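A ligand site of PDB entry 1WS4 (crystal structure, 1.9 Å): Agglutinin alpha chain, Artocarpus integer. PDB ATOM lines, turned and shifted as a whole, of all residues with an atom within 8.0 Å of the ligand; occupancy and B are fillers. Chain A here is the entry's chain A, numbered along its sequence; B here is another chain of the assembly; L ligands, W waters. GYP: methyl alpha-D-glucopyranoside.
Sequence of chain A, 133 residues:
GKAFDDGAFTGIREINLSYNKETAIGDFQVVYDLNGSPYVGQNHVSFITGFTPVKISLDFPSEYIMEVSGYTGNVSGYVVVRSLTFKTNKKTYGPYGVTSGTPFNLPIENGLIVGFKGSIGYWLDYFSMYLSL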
ATOM      1  N   GLY A   1       7.383  -7.360   0.925  1.00  0.00           N
ATOM      2  CA  GLY A   1       7.841  -8.450   1.821  1.00  0.00           C
ATOM      3  C   GLY A   1       8.273  -7.921   3.174  1.00  0.00           C
ATOM      4  O   GLY A   1       8.046  -6.749   3.489  1.00  0.00           O
ATOM      5  N   LYS A   2       8.885  -8.778   3.986  1.00  0.00           N
ATOM      6  CA  LYS A   2       9.326  -8.369   5.305  1.00  0.00           C
ATOM      7  C   LYS A   2      10.761  -7.858   5.226  1.00  0.00           C
ATOM      8  O   LYS A   2      11.672  -8.578   4.834  1.00  0.00           O
ATOM      9  CB  LYS A   2       9.272  -9.544   6.285  1.00  0.00           C
ATOM     10  CG  LYS A   2       9.580  -9.147   7.725  1.00  0.00           C
ATOM     11  CD  LYS A   2       9.579 -10.334   8.666  1.00  0.00           C
ATOM     12  CE  LYS A   2       9.862  -9.890  10.103  1.00  0.00           C
ATOM     13  NZ  LYS A   2       9.961 -11.042  11.040  1.00  0.00           N
ATOM     14  N   ALA A  24      13.045 -17.146  -8.599  1.00  0.00           N
ATOM     15  CA  ALA A  24      13.998 -16.180  -8.077  1.00  0.00           C
ATOM     16  C   ALA A  24      14.670 -16.628  -6.777  1.00  0.00           C
ATOM     17  O   ALA A  24      14.521 -17.779  -6.348  1.00  0.00           O
ATOM     18  CB  ALA A  24      13.289 -14.852  -7.847  1.00  0.00           C
ATOM     19  N   ILE A  25      15.411 -15.720  -6.157  1.00  0.00           N
ATOM     20  CA  ILE A  25      16.103 -16.010  -4.907  1.00  0.00           C
ATOM     21  C   ILE A  25      15.105 -16.027  -3.755  1.00  0.00           C
ATOM     22  O   ILE A  25      14.192 -15.191  -3.704  1.00  0.00           O
ATOM     23  CB  ILE A  25      17.176 -14.943  -4.643  1.00  0.00           C
ATOM     24  CG1 ILE A  25      18.272 -15.087  -5.699  1.00  0.00           C
ATOM     25  CG2 ILE A  25      17.732 -15.087  -3.225  1.00  0.00           C
ATOM     26  CD1 ILE A  25      19.110 -13.872  -5.848  1.00  0.00           C
ATOM     27  N   SER A  46      12.003 -17.024   3.093  1.00  0.00           N
ATOM     28  CA  SER A  46      10.926 -16.759   2.155  1.00  0.00           C
ATOM     29  C   SER A  46       9.632 -17.220   2.809  1.00  0.00           C
ATOM     30  O   SER A  46       9.655 -18.077   3.699  1.00  0.00           O
ATOM     31  CB  SER A  46      11.153 -17.570   0.873  1.00  0.00           C
ATOM     32  OG  SER A  46       9.956 -17.697   0.130  1.00  0.00           O
ATOM     33  N   PHE A  47       8.499 -16.649   2.381  1.00  0.00           N
ATOM     34  CA  PHE A  47       7.202 -17.043   2.943  1.00  0.00           C
ATOM     35  C   PHE A  47       6.811 -18.430   2.458  1.00  0.00           C
ATOM     36  O   PHE A  47       5.965 -19.089   3.066  1.00  0.00           O
ATOM     37  CB  PHE A  47       6.097 -16.064   2.536  1.00  0.00           C
ATOM     38  CG  PHE A  47       6.283 -14.661   3.060  1.00  0.00           C
ATOM     39  CD1 PHE A  47       7.123 -14.397   4.142  1.00  0.00           C
ATOM     40  CD2 PHE A  47       5.593 -13.601   2.477  1.00  0.00           C
ATOM     41  CE1 PHE A  47       7.251 -13.101   4.652  1.00  0.00           C
ATOM     42  CE2 PHE A  47       5.720 -12.298   2.968  1.00  0.00           C
ATOM     43  CZ  PHE A  47       6.552 -12.055   4.054  1.00  0.00           C
ATOM     44  N   ILE A  48       7.411 -18.879   1.362  1.00  0.00           N
ATOM     45  CA  ILE A  48       7.111 -20.191   0.802  1.00  0.00           C
ATOM     46  C   ILE A  48       8.339 -21.092   0.804  1.00  0.00           C
ATOM     47  O   ILE A  48       9.421 -20.667   1.205  1.00  0.00           O
ATOM     48  CB  ILE A  48       6.569 -20.082  -0.641  1.00  0.00           C
ATOM     49  CG1 ILE A  48       7.593 -19.357  -1.523  1.00  0.00           C
ATOM     50  CG2 ILE A  48       5.237 -19.326  -0.647  1.00  0.00           C
ATOM     51  CD1 ILE A  48       7.199 -19.273  -2.995  1.00  0.00           C
ATOM     52  N   VAL A  75       8.318 -11.573 -11.406  1.00  0.00           N
ATOM     53  CA  VAL A  75       7.922 -12.933 -11.071  1.00  0.00           C
ATOM     54  C   VAL A  75       6.477 -12.579 -10.728  1.00  0.00           C
ATOM     55  O   VAL A  75       6.221 -11.923  -9.704  1.00  0.00           O
ATOM     56  CB  VAL A  75       8.650 -13.498  -9.849  1.00  0.00           C
ATOM     57  CG1 VAL A  75       8.026 -14.827  -9.457  1.00  0.00           C
ATOM     58  CG2 VAL A  75      10.123 -13.703 -10.193  1.00  0.00           C
ATOM     59  N   SER A  76       5.560 -12.985 -11.590  1.00  0.00           N
ATOM     60  CA  SER A  76       4.164 -12.600 -11.441  1.00  0.00           C
ATOM     61  C   SER A  76       4.219 -11.076 -11.568  1.00  0.00           C
ATOM     62  O   SER A  76       4.942 -10.564 -12.426  1.00  0.00           O
ATOM     63  CB  SER A  76       3.591 -13.047 -10.099  1.00  0.00           C
ATOM     64  OG  SER A  76       3.322 -14.449 -10.128  1.00  0.00           O
ATOM     65  N   GLY A  77       3.495 -10.341 -10.733  1.00  0.00           N
ATOM     66  CA  GLY A  77       3.532  -8.892 -10.855  1.00  0.00           C
ATOM     67  C   GLY A  77       4.646  -8.176 -10.125  1.00  0.00           C
ATOM     68  O   GLY A  77       4.873  -6.976 -10.328  1.00  0.00           O
ATOM     69  N   TYR A  78       5.391  -8.906  -9.295  1.00  0.00           N
ATOM     70  CA  TYR A  78       6.457  -8.320  -8.492  1.00  0.00           C
ATOM     71  C   TYR A  78       7.846  -8.244  -9.102  1.00  0.00           C
ATOM     72  O   TYR A  78       8.293  -9.185  -9.761  1.00  0.00           O
ATOM     73  CB  TYR A  78       6.550  -9.069  -7.162  1.00  0.00           C
ATOM     74  CG  TYR A  78       5.259  -9.075  -6.384  1.00  0.00           C
ATOM     75  CD1 TYR A  78       4.908  -7.996  -5.583  1.00  0.00           C
ATOM     76  CD2 TYR A  78       4.382 -10.156  -6.472  1.00  0.00           C
ATOM     77  CE1 TYR A  78       3.707  -7.985  -4.879  1.00  0.00           C
ATOM     78  CE2 TYR A  78       3.167 -10.146  -5.778  1.00  0.00           C
ATOM     79  CZ  TYR A  78       2.839  -9.062  -4.988  1.00  0.00           C
ATOM     80  OH  TYR A  78       1.641  -9.057  -4.307  1.00  0.00           O
ATOM     81  N   VAL A  79       8.534  -7.136  -8.864  1.00  0.00           N
ATOM     82  CA  VAL A  79       9.901  -6.991  -9.340  1.00  0.00           C
ATOM     83  C   VAL A  79      10.756  -7.533  -8.192  1.00  0.00           C
ATOM     84  O   VAL A  79      10.632  -7.070  -7.055  1.00  0.00           O
ATOM     85  CB  VAL A  79      10.290  -5.520  -9.613  1.00  0.00           C
ATOM     86  CG1 VAL A  79      11.779  -5.417  -9.898  1.00  0.00           C
ATOM     87  CG2 VAL A  79       9.510  -4.985 -10.810  1.00  0.00           C
ATOM     88  N   VAL A  80      11.604  -8.509  -8.493  1.00  0.00           N
ATOM     89  CA  VAL A  80      12.449  -9.121  -7.466  1.00  0.00           C
ATOM     90  C   VAL A  80      13.851  -9.404  -7.994  1.00  0.00           C
ATOM     91  O   VAL A  80      14.141  -9.146  -9.165  1.00  0.00           O
ATOM     92  CB  VAL A  80      11.851 -10.459  -6.982  1.00  0.00           C
ATOM     93  CG1 VAL A  80      10.468 -10.226  -6.367  1.00  0.00           C
ATOM     94  CG2 VAL A  80      11.737 -11.437  -8.145  1.00  0.00           C
ATOM     95  N   VAL A  81      14.706  -9.911  -7.121  1.00  0.00           N
ATOM     96  CA  VAL A  81      16.073 -10.269  -7.515  1.00  0.00           C
ATOM     97  C   VAL A  81      15.982 -11.718  -7.966  1.00  0.00           C
ATOM     98  O   VAL A  81      15.798 -12.613  -7.153  1.00  0.00           O
ATOM     99  CB  VAL A  81      17.049 -10.150  -6.334  1.00  0.00           C
ATOM    100  CG1 VAL A  81      18.438 -10.599  -6.763  1.00  0.00           C
ATOM    101  CG2 VAL A  81      17.102  -8.708  -5.841  1.00  0.00           C
ATOM    102  N   SER A 119      14.684  -6.952   1.699  1.00  0.00           N
ATOM    103  CA  SER A 119      13.319  -7.371   1.989  1.00  0.00           C
ATOM    104  C   SER A 119      13.019  -8.694   1.287  1.00  0.00           C
ATOM    105  O   SER A 119      13.412  -8.903   0.152  1.00  0.00           O
ATOM    106  CB  SER A 119      12.341  -6.294   1.524  1.00  0.00           C
ATOM    107  OG  SER A 119      10.994  -6.727   1.659  1.00  0.00           O
ATOM    108  N   ILE A 120      12.319  -9.580   1.985  1.00  0.00           N
ATOM    109  CA  ILE A 120      11.964 -10.864   1.418  1.00  0.00           C
ATOM    110  C   ILE A 120      10.511 -11.227   1.701  1.00  0.00           C
ATOM    111  O   ILE A 120      10.058 -11.144   2.847  1.00  0.00           O
ATOM    112  CB  ILE A 120      12.855 -11.996   1.995  1.00  0.00           C
ATOM    113  CG1 ILE A 120      14.315 -11.753   1.614  1.00  0.00           C
ATOM    114  CG2 ILE A 120      12.388 -13.350   1.452  1.00  0.00           C
ATOM    115  CD1 ILE A 120      15.291 -12.771   2.217  1.00  0.00           C
ATOM    116  N   GLY A 121       9.791 -11.593   0.649  1.00  0.00           N
ATOM    117  CA  GLY A 121       8.403 -12.017   0.779  1.00  0.00           C
ATOM    118  C   GLY A 121       8.451 -13.438   0.255  1.00  0.00           C
ATOM    119  O   GLY A 121       9.021 -14.310   0.894  1.00  0.00           O
ATOM    120  N   TYR A 122       7.858 -13.677  -0.907  1.00  0.00           N
ATOM    121  CA  TYR A 122       7.929 -15.001  -1.514  1.00  0.00           C
ATOM    122  C   TYR A 122       9.372 -15.109  -2.034  1.00  0.00           C
ATOM    123  O   TYR A 122       9.973 -16.176  -2.023  1.00  0.00           O
ATOM    124  CB  TYR A 122       6.953 -15.123  -2.685  1.00  0.00           C
ATOM    125  CG  TYR A 122       5.580 -15.622  -2.285  1.00  0.00           C
ATOM    126  CD1 TYR A 122       5.096 -15.444  -0.997  1.00  0.00           C
ATOM    127  CD2 TYR A 122       4.758 -16.268  -3.221  1.00  0.00           C
ATOM    128  CE1 TYR A 122       3.816 -15.882  -0.634  1.00  0.00           C
ATOM    129  CE2 TYR A 122       3.487 -16.707  -2.869  1.00  0.00           C
ATOM    130  CZ  TYR A 122       3.021 -16.516  -1.576  1.00  0.00           C
ATOM    131  OH  TYR A 122       1.773 -16.956  -1.216  1.00  0.00           O
ATOM    132  N   TRP A 123       9.906 -13.973  -2.481  1.00  0.00           N
ATOM    133  CA  TRP A 123      11.272 -13.914  -3.009  1.00  0.00           C
ATOM    134  C   TRP A 123      11.994 -12.670  -2.500  1.00  0.00           C
ATOM    135  O   TRP A 123      11.390 -11.813  -1.851  1.00  0.00           O
ATOM    136  CB  TRP A 123      11.233 -13.896  -4.548  1.00  0.00           C
ATOM    137  CG  TRP A 123      10.435 -15.029  -5.108  1.00  0.00           C
ATOM    138  CD1 TRP A 123      10.792 -16.347  -5.143  1.00  0.00           C
ATOM    139  CD2 TRP A 123       9.085 -14.962  -5.590  1.00  0.00           C
ATOM    140  NE1 TRP A 123       9.735 -17.107  -5.615  1.00  0.00           N
ATOM    141  CE2 TRP A 123       8.683 -16.276  -5.899  1.00  0.00           C
ATOM    142  CE3 TRP A 123       8.173 -13.913  -5.791  1.00  0.00           C
ATOM    143  CZ2 TRP A 123       7.403 -16.575  -6.391  1.00  0.00           C
ATOM    144  CZ3 TRP A 123       6.906 -14.207  -6.283  1.00  0.00           C
ATOM    145  CH2 TRP A 123       6.536 -15.531  -6.576  1.00  0.00           C
ATOM    146  N   LEU A 124      13.291 -12.578  -2.789  1.00  0.00           N
ATOM    147  CA  LEU A 124      14.082 -11.412  -2.386  1.00  0.00           C
ATOM    148  C   LEU A 124      13.634 -10.219  -3.224  1.00  0.00           C
ATOM    149  O   LEU A 124      13.941 -10.126  -4.413  1.00  0.00           O
ATOM    150  CB  LEU A 124      15.567 -11.692  -2.630  1.00  0.00           C
ATOM    151  CG  LEU A 124      16.585 -10.592  -2.319  1.00  0.00           C
ATOM    152  CD1 LEU A 124      16.523 -10.205  -0.840  1.00  0.00           C
ATOM    153  CD2 LEU A 124      17.962 -11.103  -2.684  1.00  0.00           C
ATOM    154  N   ASP A 125      12.882  -9.306  -2.599  1.00  0.00           N
ATOM    155  CA  ASP A 125      12.361  -8.111  -3.271  1.00  0.00           C
ATOM    156  C   ASP A 125      13.461  -7.141  -3.685  1.00  0.00           C
ATOM    157  O   ASP A 125      13.447  -6.606  -4.800  1.00  0.00           O
ATOM    158  CB  ASP A 125      11.397  -7.362  -2.342  1.00  0.00           C
ATOM    159  CG  ASP A 125      10.213  -8.210  -1.932  1.00  0.00           C
ATOM    160  OD1 ASP A 125       9.531  -8.751  -2.827  1.00  0.00           O
ATOM    161  OD2 ASP A 125       9.967  -8.330  -0.714  1.00  0.00           O
ATOM    162  N   TYR A 126      14.380  -6.892  -2.773  1.00  0.00           N
ATOM    163  CA  TYR A 126      15.485  -5.986  -3.040  1.00  0.00           C
ATOM    164  C   TYR A 126      16.513  -6.111  -1.930  1.00  0.00           C
ATOM    165  O   TYR A 126      16.231  -6.692  -0.879  1.00  0.00           O
ATOM    166  CB  TYR A 126      14.973  -4.536  -3.107  1.00  0.00           C
ATOM    167  CG  TYR A 126      14.309  -4.034  -1.838  1.00  0.00           C
ATOM    168  CD1 TYR A 126      15.065  -3.631  -0.743  1.00  0.00           C
ATOM    169  CD2 TYR A 126      12.911  -3.977  -1.745  1.00  0.00           C
ATOM    170  CE1 TYR A 126      14.450  -3.177   0.430  1.00  0.00           C
ATOM    171  CE2 TYR A 126      12.292  -3.532  -0.575  1.00  0.00           C
ATOM    172  CZ  TYR A 126      13.066  -3.133   0.507  1.00  0.00           C
ATOM    173  OH  TYR A 126      12.460  -2.700   1.662  1.00  0.00           O
ATOM    174  N   ALA B  17      13.056  -4.293  -6.393  1.00  0.00           N
ATOM    175  CA  ALA B  17      11.846  -3.481  -6.397  1.00  0.00           C
ATOM    176  C   ALA B  17      12.095  -2.066  -5.861  1.00  0.00           C
ATOM    177  O   ALA B  17      12.942  -1.858  -5.002  1.00  0.00           O
ATOM    178  CB  ALA B  17      10.759  -4.165  -5.581  1.00  0.00           C
HETATM  179  C1  GYP L   1       4.495 -11.901  -1.678  1.00  0.00           C
HETATM  180  C2  GYP L   1       4.533 -10.780  -0.629  1.00  0.00           C
HETATM  181  C3  GYP L   1       4.943  -9.440  -1.229  1.00  0.00           C
HETATM  182  C4  GYP L   1       6.325  -9.605  -1.872  1.00  0.00           C
HETATM  183  C5  GYP L   1       6.238 -10.687  -2.968  1.00  0.00           C
HETATM  184  C6  GYP L   1       7.580 -10.912  -3.685  1.00  0.00           C
HETATM  185  C7  GYP L   1       3.336 -12.821  -3.590  1.00  0.00           C
HETATM  186  O1  GYP L   1       3.401 -11.756  -2.617  1.00  0.00           O
HETATM  187  O2  GYP L   1       3.239 -10.685  -0.006  1.00  0.00           O
HETATM  188  O3  GYP L   1       4.974  -8.441  -0.182  1.00  0.00           O
HETATM  189  O4  GYP L   1       6.737  -8.360  -2.433  1.00  0.00           O
HETATM  190  O5  GYP L   1       5.789 -11.960  -2.374  1.00  0.00           O
HETATM  191  O6  GYP L   1       8.570 -11.381  -2.774  1.00  0.00           O
HETATM  192  O   HOH W   1       5.680  -5.714  -1.912  1.00  0.00           O
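The backbone NH (N) of Gly 1 lies within hydrogen-bond range of the side-chain carboxylate (OD2) of Asp 125, 3.2 Å away.
N of Asp 125 sits at hydrogen-bond distance from O of Ser 119 (2.8 Å).
The backbone carbonyl oxygen of Asp 125 is in hydrogen-bond range of the backbone NH of Ala 17 of chain B, 2.8 Å away.
O of Gly 1 lies close to OG of Ser 119, 3.5 Å away.
The side-chain hydroxyl (OG) of Ser 46 sits at hydrogen-bond distance from the backbone carbonyl oxygen (O) of Tyr 122, at 2.6 Å.
The backbone carbonyl oxygen (O) of Gly 121 lies within hydrogen-bond range of the backbone NH (N) of Phe 47 (2.8 Å).
Residues that only touch the ligand: Tyr 78 (3.5 Å) and Gly 121 (3.6 Å).
Hydrophobic or aromatic side chains that line the ligand: Tyr 78, Tyr 122 and Trp 123.
Along chain A the residues within 4 Å of the ligand span positions 1 to 125.
The side-chain carboxylate (OD1) of Asp 125 sits at hydrogen-bond distance from an oxygen (O6) of the ligand (2.8 Å).
N of Gly 1 lies within hydrogen-bond range of O3 of the ligand (2.9 Å).
O6 of the ligand is in hydrogen-bond range of N of Trp 123 (2.9 Å).
O of Trp 123 lies within hydrogen-bond range of O6 of the ligand.
N of Tyr 122 lies within hydrogen-bond range of O6 of the ligand (3.0 Å).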
